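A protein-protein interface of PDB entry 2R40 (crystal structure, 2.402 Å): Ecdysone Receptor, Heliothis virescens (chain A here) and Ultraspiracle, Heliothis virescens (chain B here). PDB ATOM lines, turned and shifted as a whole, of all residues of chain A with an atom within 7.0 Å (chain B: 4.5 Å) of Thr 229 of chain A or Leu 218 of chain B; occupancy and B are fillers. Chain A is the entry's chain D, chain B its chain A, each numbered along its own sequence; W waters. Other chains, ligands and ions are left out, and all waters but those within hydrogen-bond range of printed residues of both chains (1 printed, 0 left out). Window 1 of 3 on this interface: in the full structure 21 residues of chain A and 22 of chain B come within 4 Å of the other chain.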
ATOM      1  N   ILE A 224       9.524 -30.211  -0.395  1.00  0.00           N
ATOM      2  CA  ILE A 224       9.648 -29.639  -1.744  1.00  0.00           C
ATOM      3  C   ILE A 224       9.608 -28.093  -1.750  1.00  0.00           C
ATOM      4  O   ILE A 224      10.431 -27.438  -2.405  1.00  0.00           O
ATOM      5  CB  ILE A 224       8.595 -30.263  -2.723  1.00  0.00           C
ATOM      6  CG1 ILE A 224       8.867 -31.761  -2.890  1.00  0.00           C
ATOM      7  CG2 ILE A 224       8.639 -29.586  -4.093  1.00  0.00           C
ATOM      8  CD1 ILE A 224       7.874 -32.510  -3.794  1.00  0.00           C
ATOM      9  N   LEU A 225       8.654 -27.515  -1.031  1.00  0.00           N
ATOM     10  CA  LEU A 225       8.553 -26.064  -0.921  1.00  0.00           C
ATOM     11  C   LEU A 225       9.759 -25.494  -0.176  1.00  0.00           C
ATOM     12  O   LEU A 225      10.118 -24.330  -0.359  1.00  0.00           O
ATOM     13  CB  LEU A 225       7.244 -25.651  -0.208  1.00  0.00           C
ATOM     14  CG  LEU A 225       5.934 -26.084  -0.892  1.00  0.00           C
ATOM     15  CD1 LEU A 225       4.690 -25.882   0.001  1.00  0.00           C
ATOM     16  CD2 LEU A 225       5.774 -25.418  -2.274  1.00  0.00           C
ATOM     17  N   GLY A 226      10.362 -26.320   0.679  1.00  0.00           N
ATOM     18  CA  GLY A 226      11.550 -25.938   1.420  1.00  0.00           C
ATOM     19  C   GLY A 226      12.730 -25.645   0.519  1.00  0.00           C
ATOM     20  O   GLY A 226      13.618 -24.907   0.901  1.00  0.00           O
ATOM     21  N   ILE A 227      12.738 -26.256  -0.662  1.00  0.00           N
ATOM     22  CA  ILE A 227      13.768 -26.069  -1.684  1.00  0.00           C
ATOM     23  C   ILE A 227      13.761 -24.655  -2.230  1.00  0.00           C
ATOM     24  O   ILE A 227      14.808 -24.103  -2.567  1.00  0.00           O
ATOM     25  CB  ILE A 227      13.574 -27.056  -2.880  1.00  0.00           C
ATOM     26  CG1 ILE A 227      13.718 -28.513  -2.399  1.00  0.00           C
ATOM     27  CG2 ILE A 227      14.548 -26.700  -4.044  1.00  0.00           C
ATOM     28  CD1 ILE A 227      13.230 -29.569  -3.392  1.00  0.00           C
ATOM     29  N   LEU A 228      12.578 -24.059  -2.298  1.00  0.00           N
ATOM     30  CA  LEU A 228      12.443 -22.705  -2.766  1.00  0.00           C
ATOM     31  C   LEU A 228      13.299 -21.755  -1.939  1.00  0.00           C
ATOM     32  O   LEU A 228      13.840 -20.766  -2.468  1.00  0.00           O
ATOM     33  CB  LEU A 228      10.976 -22.260  -2.712  1.00  0.00           C
ATOM     34  CG  LEU A 228       9.945 -22.942  -3.615  1.00  0.00           C
ATOM     35  CD1 LEU A 228       8.566 -22.347  -3.326  1.00  0.00           C
ATOM     36  CD2 LEU A 228      10.316 -22.764  -5.088  1.00  0.00           C
ATOM     37  N   THR A 229      13.407 -22.041  -0.639  1.00  0.00           N
ATOM     38  CA  THR A 229      14.152 -21.147   0.257  1.00  0.00           C
ATOM     39  C   THR A 229      15.668 -21.335   0.191  1.00  0.00           C
ATOM     40  O   THR A 229      16.390 -20.366   0.207  1.00  0.00           O
ATOM     41  CB  THR A 229      13.525 -21.028   1.711  1.00  0.00           C
ATOM     42  OG1 THR A 229      14.535 -20.860   2.723  1.00  0.00           O
ATOM     43  CG2 THR A 229      12.680 -22.152   2.025  1.00  0.00           C
ATOM     44  N   GLU A 230      16.127 -22.575   0.037  1.00  0.00           N
ATOM     45  CA  GLU A 230      17.559 -22.869  -0.094  1.00  0.00           C
ATOM     46  C   GLU A 230      18.158 -22.420  -1.435  1.00  0.00           C
ATOM     47  O   GLU A 230      19.329 -22.056  -1.500  1.00  0.00           O
ATOM     48  CB  GLU A 230      17.855 -24.358   0.172  1.00  0.00           C
ATOM     49  CG  GLU A 230      17.435 -24.872   1.572  1.00  0.00           C
ATOM     50  CD  GLU A 230      17.956 -24.031   2.732  1.00  0.00           C
ATOM     51  OE1 GLU A 230      19.155 -23.659   2.725  1.00  0.00           O
ATOM     52  OE2 GLU A 230      17.165 -23.742   3.672  1.00  0.00           O
ATOM     53  N   ILE A 231      17.370 -22.416  -2.497  1.00  0.00           N
ATOM     54  CA  ILE A 231      17.866 -21.864  -3.759  1.00  0.00           C
ATOM     55  C   ILE A 231      17.963 -20.321  -3.810  1.00  0.00           C
ATOM     56  O   ILE A 231      18.620 -19.781  -4.713  1.00  0.00           O
ATOM     57  CB  ILE A 231      17.107 -22.410  -4.978  1.00  0.00           C
ATOM     58  CG1 ILE A 231      15.635 -21.988  -4.969  1.00  0.00           C
ATOM     59  CG2 ILE A 231      17.289 -23.949  -5.105  1.00  0.00           C
ATOM     60  CD1 ILE A 231      14.867 -22.488  -6.169  1.00  0.00           C
ATOM     61  N   ARG A 232      17.331 -19.611  -2.864  1.00  0.00           N
ATOM     62  CA  ARG A 232      17.514 -18.153  -2.773  1.00  0.00           C
ATOM     63  C   ARG A 232      18.946 -17.813  -2.295  1.00  0.00           C
ATOM     64  O   ARG A 232      19.582 -16.917  -2.818  1.00  0.00           O
ATOM     65  CB  ARG A 232      16.457 -17.474  -1.860  1.00  0.00           C
ATOM     66  CG  ARG A 232      14.996 -17.936  -2.039  1.00  0.00           C
ATOM     67  CD  ARG A 232      14.324 -17.423  -3.326  1.00  0.00           C
ATOM     68  NE  ARG A 232      13.958 -16.037  -3.153  1.00  0.00           N
ATOM     69  CZ  ARG A 232      12.738 -15.525  -3.235  1.00  0.00           C
ATOM     70  NH1 ARG A 232      11.667 -16.252  -3.571  1.00  0.00           N
ATOM     71  NH2 ARG A 232      12.621 -14.241  -3.003  1.00  0.00           N
ATOM     72  N   THR A 233      19.451 -18.564  -1.323  1.00  0.00           N
ATOM     73  CA  THR A 233      20.852 -18.493  -0.917  1.00  0.00           C
ATOM     74  C   THR A 233      21.827 -18.776  -2.062  1.00  0.00           C
ATOM     75  O   THR A 233      22.748 -17.984  -2.286  1.00  0.00           O
ATOM     76  CB  THR A 233      21.145 -19.458   0.229  1.00  0.00           C
ATOM     77  OG1 THR A 233      20.195 -19.230   1.264  1.00  0.00           O
ATOM     78  CG2 THR A 233      22.535 -19.249   0.792  1.00  0.00           C
ATOM     79  N   LEU A 234      21.630 -19.892  -2.771  1.00  0.00           N
ATOM     80  CA  LEU A 234      22.518 -20.260  -3.862  1.00  0.00           C
ATOM     81  C   LEU A 234      22.493 -19.263  -5.016  1.00  0.00           C
ATOM     82  O   LEU A 234      23.551 -18.941  -5.584  1.00  0.00           O
ATOM     83  CB  LEU A 234      22.214 -21.657  -4.378  1.00  0.00           C
ATOM     84  CG  LEU A 234      22.380 -22.823  -3.403  1.00  0.00           C
ATOM     85  CD1 LEU A 234      21.718 -24.066  -4.003  1.00  0.00           C
ATOM     86  CD2 LEU A 234      23.830 -23.102  -3.055  1.00  0.00           C
ATOM     87  N   LEU B 166       5.508 -21.337  11.874  1.00  0.00           N
ATOM     88  CA  LEU B 166       6.527 -20.953  10.882  1.00  0.00           C
ATOM     89  C   LEU B 166       7.888 -20.638  11.509  1.00  0.00           C
ATOM     90  O   LEU B 166       8.920 -20.966  10.940  1.00  0.00           O
ATOM     91  CB  LEU B 166       6.036 -19.795  10.009  1.00  0.00           C
ATOM     92  CG  LEU B 166       4.878 -20.160   9.063  1.00  0.00           C
ATOM     93  CD1 LEU B 166       4.134 -18.905   8.607  1.00  0.00           C
ATOM     94  CD2 LEU B 166       5.344 -21.017   7.854  1.00  0.00           C
ATOM     95  N   ILE B 169       9.530 -23.922  12.211  1.00  0.00           N
ATOM     96  CA  ILE B 169       9.969 -24.476  10.935  1.00  0.00           C
ATOM     97  C   ILE B 169      11.238 -23.767  10.449  1.00  0.00           C
ATOM     98  O   ILE B 169      12.140 -24.414   9.899  1.00  0.00           O
ATOM     99  CB  ILE B 169       8.872 -24.361   9.863  1.00  0.00           C
ATOM    100  CG1 ILE B 169       7.706 -25.284  10.207  1.00  0.00           C
ATOM    101  CG2 ILE B 169       9.438 -24.695   8.474  1.00  0.00           C
ATOM    102  CD1 ILE B 169       6.436 -25.056   9.362  1.00  0.00           C
ATOM    103  N   ILE B 170      11.303 -22.449  10.643  1.00  0.00           N
ATOM    104  CA  ILE B 170      12.491 -21.670  10.278  1.00  0.00           C
ATOM    105  C   ILE B 170      13.725 -22.167  11.025  1.00  0.00           C
ATOM    106  O   ILE B 170      14.756 -22.430  10.415  1.00  0.00           O
ATOM    107  CB  ILE B 170      12.316 -20.140  10.539  1.00  0.00           C
ATOM    108  CG1 ILE B 170      11.221 -19.554   9.641  1.00  0.00           C
ATOM    109  CG2 ILE B 170      13.676 -19.371  10.319  1.00  0.00           C
ATOM    110  CD1 ILE B 170      10.672 -18.225  10.125  1.00  0.00           C
ATOM    111  N   LEU B 215       3.940 -21.069   3.489  1.00  0.00           N
ATOM    112  CA  LEU B 215       5.337 -21.486   3.291  1.00  0.00           C
ATOM    113  C   LEU B 215       6.070 -20.707   2.206  1.00  0.00           C
ATOM    114  O   LEU B 215       7.291 -20.720   2.178  1.00  0.00           O
ATOM    115  CB  LEU B 215       5.431 -22.995   3.037  1.00  0.00           C
ATOM    116  CG  LEU B 215       4.959 -23.925   4.172  1.00  0.00           C
ATOM    117  CD1 LEU B 215       4.918 -25.365   3.683  1.00  0.00           C
ATOM    118  CD2 LEU B 215       5.848 -23.821   5.410  1.00  0.00           C
ATOM    119  N   LEU B 216       5.332 -20.032   1.326  1.00  0.00           N
ATOM    120  CA  LEU B 216       5.911 -19.129   0.321  1.00  0.00           C
ATOM    121  C   LEU B 216       6.518 -17.867   0.912  1.00  0.00           C
ATOM    122  O   LEU B 216       7.178 -17.114   0.204  1.00  0.00           O
ATOM    123  CB  LEU B 216       4.852 -18.714  -0.700  1.00  0.00           C
ATOM    124  CG  LEU B 216       4.792 -19.375  -2.081  1.00  0.00           C
ATOM    125  CD1 LEU B 216       5.286 -20.809  -2.074  1.00  0.00           C
ATOM    126  CD2 LEU B 216       3.357 -19.288  -2.605  1.00  0.00           C
ATOM    127  N   ARG B 217       6.285 -17.623   2.196  1.00  0.00           N
ATOM    128  CA  ARG B 217       6.836 -16.448   2.874  1.00  0.00           C
ATOM    129  C   ARG B 217       8.306 -16.653   3.233  1.00  0.00           C
ATOM    130  O   ARG B 217       9.081 -15.695   3.335  1.00  0.00           O
ATOM    131  CB  ARG B 217       6.020 -16.131   4.138  1.00  0.00           C
ATOM    132  CG  ARG B 217       4.558 -15.778   3.889  1.00  0.00           C
ATOM    133  CD  ARG B 217       4.421 -14.650   2.886  1.00  0.00           C
ATOM    134  NE  ARG B 217       4.130 -15.104   1.527  1.00  0.00           N
ATOM    135  CZ  ARG B 217       4.626 -14.536   0.424  1.00  0.00           C
ATOM    136  NH1 ARG B 217       5.477 -13.493   0.500  1.00  0.00           N
ATOM    137  NH2 ARG B 217       4.289 -15.024  -0.767  1.00  0.00           N
ATOM    138  N   LEU B 218       8.660 -17.924   3.392  1.00  0.00           N
ATOM    139  CA  LEU B 218       9.958 -18.373   3.869  1.00  0.00           C
ATOM    140  C   LEU B 218      11.116 -18.073   2.892  1.00  0.00           C
ATOM    141  O   LEU B 218      12.152 -17.576   3.320  1.00  0.00           O
ATOM    142  CB  LEU B 218       9.868 -19.862   4.267  1.00  0.00           C
ATOM    143  CG  LEU B 218       9.605 -20.236   5.751  1.00  0.00           C
ATOM    144  CD1 LEU B 218       8.635 -19.308   6.488  1.00  0.00           C
ATOM    145  CD2 LEU B 218       9.181 -21.689   5.942  1.00  0.00           C
ATOM    146  N   PRO B 219      10.948 -18.365   1.582  1.00  0.00           N
ATOM    147  CA  PRO B 219      11.961 -17.938   0.613  1.00  0.00           C
ATOM    148  C   PRO B 219      12.152 -16.414   0.574  1.00  0.00           C
ATOM    149  O   PRO B 219      13.302 -15.928   0.490  1.00  0.00           O
ATOM    150  CB  PRO B 219      11.404 -18.437  -0.729  1.00  0.00           C
ATOM    151  CG  PRO B 219      10.456 -19.528  -0.381  1.00  0.00           C
ATOM    152  CD  PRO B 219       9.871 -19.151   0.937  1.00  0.00           C
ATOM    153  N   ALA B 220      11.036 -15.680   0.603  1.00  0.00           N
ATOM    154  CA  ALA B 220      11.058 -14.212   0.667  1.00  0.00           C
ATOM    155  C   ALA B 220      11.864 -13.726   1.878  1.00  0.00           C
ATOM    156  O   ALA B 220      12.681 -12.830   1.756  1.00  0.00           O
ATOM    157  CB  ALA B 220       9.625 -13.652   0.719  1.00  0.00           C
ATOM    158  N   LEU B 221      11.615 -14.332   3.036  1.00  0.00           N
ATOM    159  CA  LEU B 221      12.344 -14.043   4.259  1.00  0.00           C
ATOM    160  C   LEU B 221      13.833 -14.391   4.147  1.00  0.00           C
ATOM    161  O   LEU B 221      14.672 -13.689   4.704  1.00  0.00           O
ATOM    162  CB  LEU B 221      11.703 -14.772   5.453  1.00  0.00           C
ATOM    163  CG  LEU B 221      12.429 -14.768   6.811  1.00  0.00           C
ATOM    164  CD1 LEU B 221      12.441 -13.370   7.437  1.00  0.00           C
ATOM    165  CD2 LEU B 221      11.789 -15.759   7.744  1.00  0.00           C
ATOM    166  N   ARG B 222      14.167 -15.449   3.414  1.00  0.00           N
ATOM    167  CA  ARG B 222      15.568 -15.801   3.193  1.00  0.00           C
ATOM    168  C   ARG B 222      16.305 -14.721   2.372  1.00  0.00           C
ATOM    169  O   ARG B 222      17.350 -14.233   2.791  1.00  0.00           O
ATOM    170  CB  ARG B 222      15.703 -17.183   2.541  1.00  0.00           C
ATOM    171  CG  ARG B 222      17.164 -17.620   2.264  1.00  0.00           C
ATOM    172  CD  ARG B 222      17.987 -17.820   3.558  1.00  0.00           C
ATOM    173  NE  ARG B 222      17.548 -18.978   4.368  1.00  0.00           N
ATOM    174  CZ  ARG B 222      17.887 -20.246   4.111  1.00  0.00           C
ATOM    175  NH1 ARG B 222      18.633 -20.536   3.047  1.00  0.00           N
ATOM    176  NH2 ARG B 222      17.483 -21.234   4.909  1.00  0.00           N
HETATM  177  O   HOH W   1       8.863 -22.821   1.837  1.00  0.00           O
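Water W1 lies within hydrogen-bond range of O of Leu 215 of chain B and O of Leu 225 of chain A.
NH2 of Arg 222 of chain B is in salt-bridge range of OE2 of Glu 230 of chain A, 2.8 Å away. The side-chain hydroxyl of Thr 233 of chain A is in hydrogen-bond range of the guanidinium group of Arg 222 of chain B, at 2.7 Å.
Of the 11 printed residues of chain A, 6 touch a printed residue of chain B. Hydrophobic or aromatic side chains of chain A within 4 Å of the printed part of chain B: Leu 225 and Leu 228. Of the 11 printed residues of chain B, 6 touch a printed residue of chain A. Printed residues of chain B that touch a printed residue of chain A: Leu 215, Leu 216, Leu 218, Pro 219, Ala 220 and Arg 222. Hydrophobic or aromatic side chains of chain B that line the printed part of chain A: Leu 215, Leu 216 and Pro 219. Among the printed residues, Asp or Glu carboxylates within 4 Å of a Lys or Arg side-chain nitrogen of the other chain: Glu 230 of chain A with Arg 222 of chain B (2.8 Å).
Of the printed residues of chain B, Thr 229 of chain A touches Leu 218 (3.99 Å), Pro 219 (3.6 Å) and Arg 222 (3.5 Å). Printed residues of chain A within 4 Å of Leu 218 of chain B: Thr 229. Of the printed residues of chain A, Pro 219 of chain B touches Leu 228, Thr 229 and Arg 232. Of the printed residues of chain B, Glu 230 of chain A touches Arg 222 (2.8 Å). Ile 224 of chain A touches none of the printed residues of chain B. The nearest printed residue of chain A that does not touch Ala 220 of chain B is Thr 229 of chain A (6.0 Å).
Leu 225 of chain A touches Leu 215 of chain B (CD1 to CD1, 3.7 Å). Leu 228 of chain A touches Leu 216 of chain B (CD1 to CD1, 3.8 Å). CB of Leu 228 of chain A touches CG of Pro 219 of chain B, 3.6 Å away. Thr 229 of chain A touches Leu 218 of chain B (CB to C, 3.99 Å). CB of Thr 229 of chain A touches CA of Pro 219 of chain B (3.6 Å). Thr 229 of chain A touches Arg 222 of chain B (O to CG, 3.5 Å). Pro 219 of chain B touches Arg 232 of chain A (CB to NH1, 3.6 Å). CA of Ala 220 of chain B touches NH2 of Arg 232 of chain A (3.99 Å).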
